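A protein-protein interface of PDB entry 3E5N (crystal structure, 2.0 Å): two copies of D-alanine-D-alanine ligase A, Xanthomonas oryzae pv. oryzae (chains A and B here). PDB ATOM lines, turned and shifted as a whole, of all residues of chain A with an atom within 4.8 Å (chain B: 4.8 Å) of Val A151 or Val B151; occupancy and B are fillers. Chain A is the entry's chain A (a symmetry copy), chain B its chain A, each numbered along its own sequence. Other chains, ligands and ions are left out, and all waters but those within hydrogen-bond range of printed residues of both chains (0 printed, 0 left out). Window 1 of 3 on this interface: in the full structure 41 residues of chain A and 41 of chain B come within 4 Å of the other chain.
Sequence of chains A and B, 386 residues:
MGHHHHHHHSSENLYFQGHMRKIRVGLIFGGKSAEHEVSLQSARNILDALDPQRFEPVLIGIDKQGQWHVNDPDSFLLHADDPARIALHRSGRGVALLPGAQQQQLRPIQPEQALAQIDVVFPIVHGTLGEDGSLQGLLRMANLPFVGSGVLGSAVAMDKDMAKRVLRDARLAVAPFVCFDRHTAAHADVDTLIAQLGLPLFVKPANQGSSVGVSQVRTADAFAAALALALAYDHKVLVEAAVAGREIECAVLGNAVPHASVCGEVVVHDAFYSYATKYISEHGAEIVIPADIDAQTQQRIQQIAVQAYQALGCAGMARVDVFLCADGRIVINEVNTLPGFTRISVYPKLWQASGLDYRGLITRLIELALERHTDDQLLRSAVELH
O of Gly B137 sits close to O of Ser A134.
The side-chain carboxylate of Asp B132 lies within salt-bridge range of the guanidinium group of Arg A140, at 2.9 Å.
NE of Arg B140 lies within hydrogen-bond range of OG of Ser A134.
NH2 of Arg B140 lies within salt-bridge range of OD1 of Asp A132 (2.9 Å).
The backbone carbonyl oxygen (O) of Ser B134 lies close to the backbone carbonyl oxygen (O) of Gly A137, at 3.4 Å.
The guanidinium group (NE) of Arg A140 sits at hydrogen-bond distance from the side-chain hydroxyl (OG) of Ser B134 (2.9 Å).
OD2 of Asp B132 lies within hydrogen-bond range of OG of Ser B134 (2.7 Å).
N of Gly B133 lies close to OE1 of Gln B136 (2.9 Å).
The side-chain hydroxyl of Ser A134 sits at hydrogen-bond distance from the side-chain carboxylate of Asp A132.
N of Gly A133 lies close to OE1 of Gln A136, at 2.9 Å.
Asp A132 touches Val B151 (O to CG1, 3.8 Å).
Gly A133 touches Val B151 (C to CG1, 3.9 Å).
Val B151 touches Ser A134.
Val A151 touches Asp B132 (CG1 to O, 3.8 Å).
C of Gly B133 touches CG1 of Val A151, at 3.9 Å.
Val A151 touches Ser B134 (CG2 to OG, 3.8 Å).
Val A151 touches Val B151 (CG1 to CG1, 3.7 Å).
C of Ala B155 touches CD1 of Leu A152, at 3.9 Å.
C of Ala A155 touches CD1 of Leu B152 (3.9 Å).
Val A151 touches four residues of chain B.
Of chain A, only Asp A132, Gly A133, Ser A134 and Val A151 come within 4 Å of Val B151.
Of the printed residues of chain B, Arg A140 touches Asp B132 and Ser B134.
Of the printed residues of chain A, Arg B140 touches Asp A132 (2.9 Å) and Ser A134 (2.9 Å).
Printed residues of chain B within 4 Å of Ser A134: Gly B137 (3.4 Å), Arg B140 (2.9 Å) and Val B151 (3.8 Å).
Gly B150 touches none of the printed residues of chain A.
Gln B136 touches none of the printed residues of chain A.
The nearest residue of chain B that does not touch Val A151 is Ala B155 (4.2 Å).
The nearest residue of chain A that does not touch Val B151 is Ala A155 (4.2 Å).
The nearest printed residue of chain A that does not touch Arg B140 is Gly A133 (6.7 Å).
Hydrophobic or aromatic side chains of chain B within 4 Å of the printed part of chain A: Val B151, Leu B152 and Ala B155.
Of the 13 printed residues of chain A, 8 touch a printed residue of chain B.
Among the printed residues, Asp or Glu carboxylates within 4 Å of a Lys or Arg side-chain nitrogen of the other chain: Asp A132 with Arg B140 (2.9 Å) and Arg A140 with Asp B132 (2.9 Å).
Asp A132 touches Arg B140, and with the chains exchanged Arg A140 touches Asp B132.
Asp A132 touches Val B151, and with the chains exchanged Val A151 touches Asp B132.
Gly A133 touches Val B151, and with the chains exchanged Val A151 touches Gly B133.
Ser A134 touches Val B151, and with the chains exchanged Val A151 touches Ser B134.
Positions printed for both chains: 132, 133, 134, 136, 137, 140, 149, 150, 151, 152, 153, 154 and 155.
Of the 15 pairs that touch across the chains among the printed residues, 15 have their exchanged pair printed and touching as well.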
ATOM      1  N   ASP A 132      18.159 -11.640  13.940  1.00  0.00           N
ATOM      2  CA  ASP A 132      18.202 -12.751  13.017  1.00  0.00           C
ATOM      3  C   ASP A 132      19.609 -12.872  12.333  1.00  0.00           C
ATOM      4  O   ASP A 132      19.755 -13.616  11.366  1.00  0.00           O
ATOM      5  CB  ASP A 132      17.060 -12.609  11.986  1.00  0.00           C
ATOM      6  CG  ASP A 132      17.351 -11.505  10.893  1.00  0.00           C
ATOM      7  OD1 ASP A 132      16.470 -11.297   9.965  1.00  0.00           O
ATOM      8  OD2 ASP A 132      18.502 -10.868  10.956  1.00  0.00           O
ATOM      9  N   GLY A 133      20.621 -12.106  12.815  1.00  0.00           N
ATOM     10  CA  GLY A 133      21.969 -12.269  12.262  1.00  0.00           C
ATOM     11  C   GLY A 133      22.317 -11.171  11.326  1.00  0.00           C
ATOM     12  O   GLY A 133      23.485 -11.093  10.926  1.00  0.00           O
ATOM     13  N   SER A 134      21.298 -10.359  10.902  1.00  0.00           N
ATOM     14  CA  SER A 134      21.593  -9.257   9.968  1.00  0.00           C
ATOM     15  C   SER A 134      22.461  -8.217  10.652  1.00  0.00           C
ATOM     16  O   SER A 134      23.422  -7.796  10.075  1.00  0.00           O
ATOM     17  CB  SER A 134      20.307  -8.565   9.409  1.00  0.00           C
ATOM     18  OG  SER A 134      19.483  -9.579   8.806  1.00  0.00           O
ATOM     19  N   GLN A 136      24.353  -8.564  13.241  1.00  0.00           N
ATOM     20  CA  GLN A 136      25.615  -9.260  13.568  1.00  0.00           C
ATOM     21  C   GLN A 136      26.537  -9.273  12.334  1.00  0.00           C
ATOM     22  O   GLN A 136      27.721  -8.966  12.444  1.00  0.00           O
ATOM     23  CB  GLN A 136      25.295 -10.717  14.081  1.00  0.00           C
ATOM     24  CG  GLN A 136      24.517 -10.819  15.469  1.00  0.00           C
ATOM     25  CD  GLN A 136      23.007 -10.340  15.431  1.00  0.00           C
ATOM     26  OE1 GLN A 136      22.339 -10.431  14.379  1.00  0.00           O
ATOM     27  NE2 GLN A 136      22.491  -9.864  16.608  1.00  0.00           N
ATOM     28  N   GLY A 137      25.949  -9.509  11.150  1.00  0.00           N
ATOM     29  CA  GLY A 137      26.693  -9.440   9.910  1.00  0.00           C
ATOM     30  C   GLY A 137      27.247  -8.064   9.636  1.00  0.00           C
ATOM     31  O   GLY A 137      28.401  -7.928   9.244  1.00  0.00           O
ATOM     32  N   ARG A 140      30.183  -7.610  12.085  1.00  0.00           N
ATOM     33  CA  ARG A 140      31.312  -8.353  11.440  1.00  0.00           C
ATOM     34  C   ARG A 140      31.962  -7.644  10.284  1.00  0.00           C
ATOM     35  O   ARG A 140      33.197  -7.597  10.203  1.00  0.00           O
ATOM     36  CB  ARG A 140      30.895  -9.749  10.989  1.00  0.00           C
ATOM     37  CG  ARG A 140      31.000 -10.711  12.159  1.00  0.00           C
ATOM     38  CD  ARG A 140      30.337 -12.026  11.846  1.00  0.00           C
ATOM     39  NE  ARG A 140      31.089 -12.808  10.843  1.00  0.00           N
ATOM     40  CZ  ARG A 140      32.269 -13.401  11.037  1.00  0.00           C
ATOM     41  NH1 ARG A 140      32.903 -13.331  12.213  1.00  0.00           N
ATOM     42  NH2 ARG A 140      32.779 -14.112  10.046  1.00  0.00           N
ATOM     43  N   SER A 149      25.234 -14.027  20.202  1.00  0.00           N
ATOM     44  CA  SER A 149      25.493 -15.030  19.162  1.00  0.00           C
ATOM     45  C   SER A 149      25.959 -14.394  17.840  1.00  0.00           C
ATOM     46  O   SER A 149      25.645 -13.272  17.541  1.00  0.00           O
ATOM     47  CB  SER A 149      24.242 -15.939  18.944  1.00  0.00           C
ATOM     48  OG  SER A 149      23.979 -16.634  20.124  1.00  0.00           O
ATOM     49  N   GLY A 150      26.808 -15.087  17.105  1.00  0.00           N
ATOM     50  CA  GLY A 150      27.215 -14.571  15.806  1.00  0.00           C
ATOM     51  C   GLY A 150      26.124 -14.672  14.759  1.00  0.00           C
ATOM     52  O   GLY A 150      24.977 -14.929  15.067  1.00  0.00           O
ATOM     53  N   VAL A 151      26.507 -14.556  13.508  1.00  0.00           N
ATOM     54  CA  VAL A 151      25.555 -14.595  12.378  1.00  0.00           C
ATOM     55  C   VAL A 151      24.747 -15.918  12.351  1.00  0.00           C
ATOM     56  O   VAL A 151      23.511 -15.891  12.402  1.00  0.00           O
ATOM     57  CB  VAL A 151      26.325 -14.301  11.048  1.00  0.00           C
ATOM     58  CG1 VAL A 151      25.412 -14.386   9.790  1.00  0.00           C
ATOM     59  CG2 VAL A 151      26.975 -12.857  11.107  1.00  0.00           C
ATOM     60  N   LEU A 152      25.443 -17.059  12.259  1.00  0.00           N
ATOM     61  CA  LEU A 152      24.828 -18.389  12.203  1.00  0.00           C
ATOM     62  C   LEU A 152      23.977 -18.669  13.390  1.00  0.00           C
ATOM     63  O   LEU A 152      22.815 -19.090  13.225  1.00  0.00           O
ATOM     64  CB  LEU A 152      25.851 -19.533  12.071  1.00  0.00           C
ATOM     65  CG  LEU A 152      25.375 -21.029  11.982  1.00  0.00           C
ATOM     66  CD1 LEU A 152      24.359 -21.274  10.884  1.00  0.00           C
ATOM     67  CD2 LEU A 152      26.526 -22.012  11.856  1.00  0.00           C
ATOM     68  N   GLY A 153      24.495 -18.480  14.608  1.00  0.00           N
ATOM     69  CA  GLY A 153      23.684 -18.859  15.752  1.00  0.00           C
ATOM     70  C   GLY A 153      22.421 -18.039  15.875  1.00  0.00           C
ATOM     71  O   GLY A 153      21.359 -18.546  16.238  1.00  0.00           O
ATOM     72  N   SER A 154      22.527 -16.761  15.584  1.00  0.00           N
ATOM     73  CA  SER A 154      21.368 -15.821  15.588  1.00  0.00           C
ATOM     74  C   SER A 154      20.324 -16.202  14.544  1.00  0.00           C
ATOM     75  O   SER A 154      19.155 -16.247  14.832  1.00  0.00           O
ATOM     76  CB  SER A 154      21.840 -14.351  15.406  1.00  0.00           C
ATOM     77  OG  SER A 154      22.780 -14.015  16.432  1.00  0.00           O
ATOM     78  N   ALA A 155      20.774 -16.430  13.317  1.00  0.00           N
ATOM     79  CA  ALA A 155      19.935 -16.778  12.184  1.00  0.00           C
ATOM     80  C   ALA A 155      19.200 -18.102  12.432  1.00  0.00           C
ATOM     81  O   ALA A 155      17.974 -18.183  12.204  1.00  0.00           O
ATOM     82  CB  ALA A 155      20.816 -16.838  10.826  1.00  0.00           C
ATOM     83  N   ASP B 132      29.394 -16.073   4.148  1.00  0.00           N
ATOM     84  CA  ASP B 132      28.880 -16.726   5.330  1.00  0.00           C
ATOM     85  C   ASP B 132      27.645 -15.956   5.918  1.00  0.00           C
ATOM     86  O   ASP B 132      27.225 -16.243   7.037  1.00  0.00           O
ATOM     87  CB  ASP B 132      30.018 -16.888   6.364  1.00  0.00           C
ATOM     88  CG  ASP B 132      30.380 -15.534   7.095  1.00  0.00           C
ATOM     89  OD1 ASP B 132      31.315 -15.541   7.993  1.00  0.00           O
ATOM     90  OD2 ASP B 132      29.685 -14.460   6.780  1.00  0.00           O
ATOM     91  N   GLY B 133      27.104 -14.957   5.176  1.00  0.00           N
ATOM     92  CA  GLY B 133      25.892 -14.286   5.655  1.00  0.00           C
ATOM     93  C   GLY B 133      26.191 -12.953   6.233  1.00  0.00           C
ATOM     94  O   GLY B 133      25.242 -12.210   6.513  1.00  0.00           O
ATOM     95  N   SER B 134      27.504 -12.660   6.494  1.00  0.00           N
ATOM     96  CA  SER B 134      27.852 -11.350   7.074  1.00  0.00           C
ATOM     97  C   SER B 134      27.554 -10.247   6.075  1.00  0.00           C
ATOM     98  O   SER B 134      26.966  -9.274   6.446  1.00  0.00           O
ATOM     99  CB  SER B 134      29.348 -11.251   7.517  1.00  0.00           C
ATOM    100  OG  SER B 134      29.615 -12.333   8.428  1.00  0.00           O
ATOM    101  N   GLN B 136      25.554 -10.310   3.546  1.00  0.00           N
ATOM    102  CA  GLN B 136      24.093 -10.360   3.329  1.00  0.00           C
ATOM    103  C   GLN B 136      23.372  -9.590   4.451  1.00  0.00           C
ATOM    104  O   GLN B 136      22.484  -8.787   4.178  1.00  0.00           O
ATOM    105  CB  GLN B 136      23.624 -11.865   3.251  1.00  0.00           C
ATOM    106  CG  GLN B 136      24.151 -12.703   2.002  1.00  0.00           C
ATOM    107  CD  GLN B 136      25.702 -13.031   2.017  1.00  0.00           C
ATOM    108  OE1 GLN B 136      26.313 -13.149   3.100  1.00  0.00           O
ATOM    109  NE2 GLN B 136      26.298 -13.204   0.796  1.00  0.00           N
ATOM    110  N   GLY B 137      23.854  -9.754   5.694  1.00  0.00           N
ATOM    111  CA  GLY B 137      23.329  -9.000   6.813  1.00  0.00           C
ATOM    112  C   GLY B 137      23.537  -7.512   6.666  1.00  0.00           C
ATOM    113  O   GLY B 137      22.628  -6.732   6.923  1.00  0.00           O
ATOM    114  N   ARG B 140      21.030  -6.364   3.981  1.00  0.00           N
ATOM    115  CA  ARG B 140      19.731  -6.257   4.720  1.00  0.00           C
ATOM    116  C   ARG B 140      19.593  -5.039   5.592  1.00  0.00           C
ATOM    117  O   ARG B 140      18.547  -4.376   5.568  1.00  0.00           O
ATOM    118  CB  ARG B 140      19.445  -7.499   5.558  1.00  0.00           C
ATOM    119  CG  ARG B 140      18.801  -8.561   4.686  1.00  0.00           C
ATOM    120  CD  ARG B 140      18.758  -9.892   5.388  1.00  0.00           C
ATOM    121  NE  ARG B 140      17.796  -9.905   6.508  1.00  0.00           N
ATOM    122  CZ  ARG B 140      16.465  -9.874   6.398  1.00  0.00           C
ATOM    123  NH1 ARG B 140      15.864  -9.823   5.203  1.00  0.00           N
ATOM    124  NH2 ARG B 140      15.747  -9.949   7.504  1.00  0.00           N
ATOM    125  N   SER B 149      21.624 -16.292  -1.731  1.00  0.00           N
ATOM    126  CA  SER B 149      20.984 -16.719  -0.481  1.00  0.00           C
ATOM    127  C   SER B 149      20.984 -15.607   0.584  1.00  0.00           C
ATOM    128  O   SER B 149      21.825 -14.748   0.591  1.00  0.00           O
ATOM    129  CB  SER B 149      21.645 -18.025   0.063  1.00  0.00           C
ATOM    130  OG  SER B 149      21.450 -19.048  -0.864  1.00  0.00           O
ATOM    131  N   GLY B 150      19.959 -15.571   1.415  1.00  0.00           N
ATOM    132  CA  GLY B 150      19.951 -14.594   2.495  1.00  0.00           C
ATOM    133  C   GLY B 150      20.925 -14.928   3.606  1.00  0.00           C
ATOM    134  O   GLY B 150      21.776 -15.784   3.461  1.00  0.00           O
ATOM    135  N   VAL B 151      20.739 -14.309   4.749  1.00  0.00           N
ATOM    136  CA  VAL B 151      21.630 -14.501   5.913  1.00  0.00           C
ATOM    137  C   VAL B 151      21.689 -15.987   6.353  1.00  0.00           C
ATOM    138  O   VAL B 151      22.774 -16.580   6.385  1.00  0.00           O
ATOM    139  CB  VAL B 151      21.197 -13.523   7.056  1.00  0.00           C
ATOM    140  CG1 VAL B 151      22.042 -13.700   8.352  1.00  0.00           C
ATOM    141  CG2 VAL B 151      21.331 -12.022   6.563  1.00  0.00           C
ATOM    142  N   LEU B 152      20.534 -16.570   6.698  1.00  0.00           N
ATOM    143  CA  LEU B 152      20.424 -17.959   7.154  1.00  0.00           C
ATOM    144  C   LEU B 152      20.944 -18.926   6.151  1.00  0.00           C
ATOM    145  O   LEU B 152      21.761 -19.798   6.507  1.00  0.00           O
ATOM    146  CB  LEU B 152      18.985 -18.374   7.515  1.00  0.00           C
ATOM    147  CG  LEU B 152      18.678 -19.825   8.038  1.00  0.00           C
ATOM    148  CD1 LEU B 152      19.520 -20.228   9.232  1.00  0.00           C
ATOM    149  CD2 LEU B 152      17.206 -20.046   8.341  1.00  0.00           C
ATOM    150  N   GLY B 153      20.497 -18.844   4.893  1.00  0.00           N
ATOM    151  CA  GLY B 153      20.936 -19.863   3.954  1.00  0.00           C
ATOM    152  C   GLY B 153      22.426 -19.831   3.706  1.00  0.00           C
ATOM    153  O   GLY B 153      23.077 -20.867   3.570  1.00  0.00           O
ATOM    154  N   SER B 154      22.977 -18.640   3.634  1.00  0.00           N
ATOM    155  CA  SER B 154      24.444 -18.425   3.460  1.00  0.00           C
ATOM    156  C   SER B 154      25.242 -18.969   4.641  1.00  0.00           C
ATOM    157  O   SER B 154      26.216 -19.653   4.459  1.00  0.00           O
ATOM    158  CB  SER B 154      24.763 -16.925   3.205  1.00  0.00           C
ATOM    159  OG  SER B 154      24.036 -16.463   2.062  1.00  0.00           O
ATOM    160  N   ALA B 155      24.826 -18.608   5.848  1.00  0.00           N
ATOM    161  CA  ALA B 155      25.468 -19.001   7.090  1.00  0.00           C
ATOM    162  C   ALA B 155      25.445 -20.526   7.261  1.00  0.00           C
ATOM    163  O   ALA B 155      26.488 -21.129   7.590  1.00  0.00           O
ATOM    164  CB  ALA B 155      24.770 -18.256   8.347  1.00  0.00           C
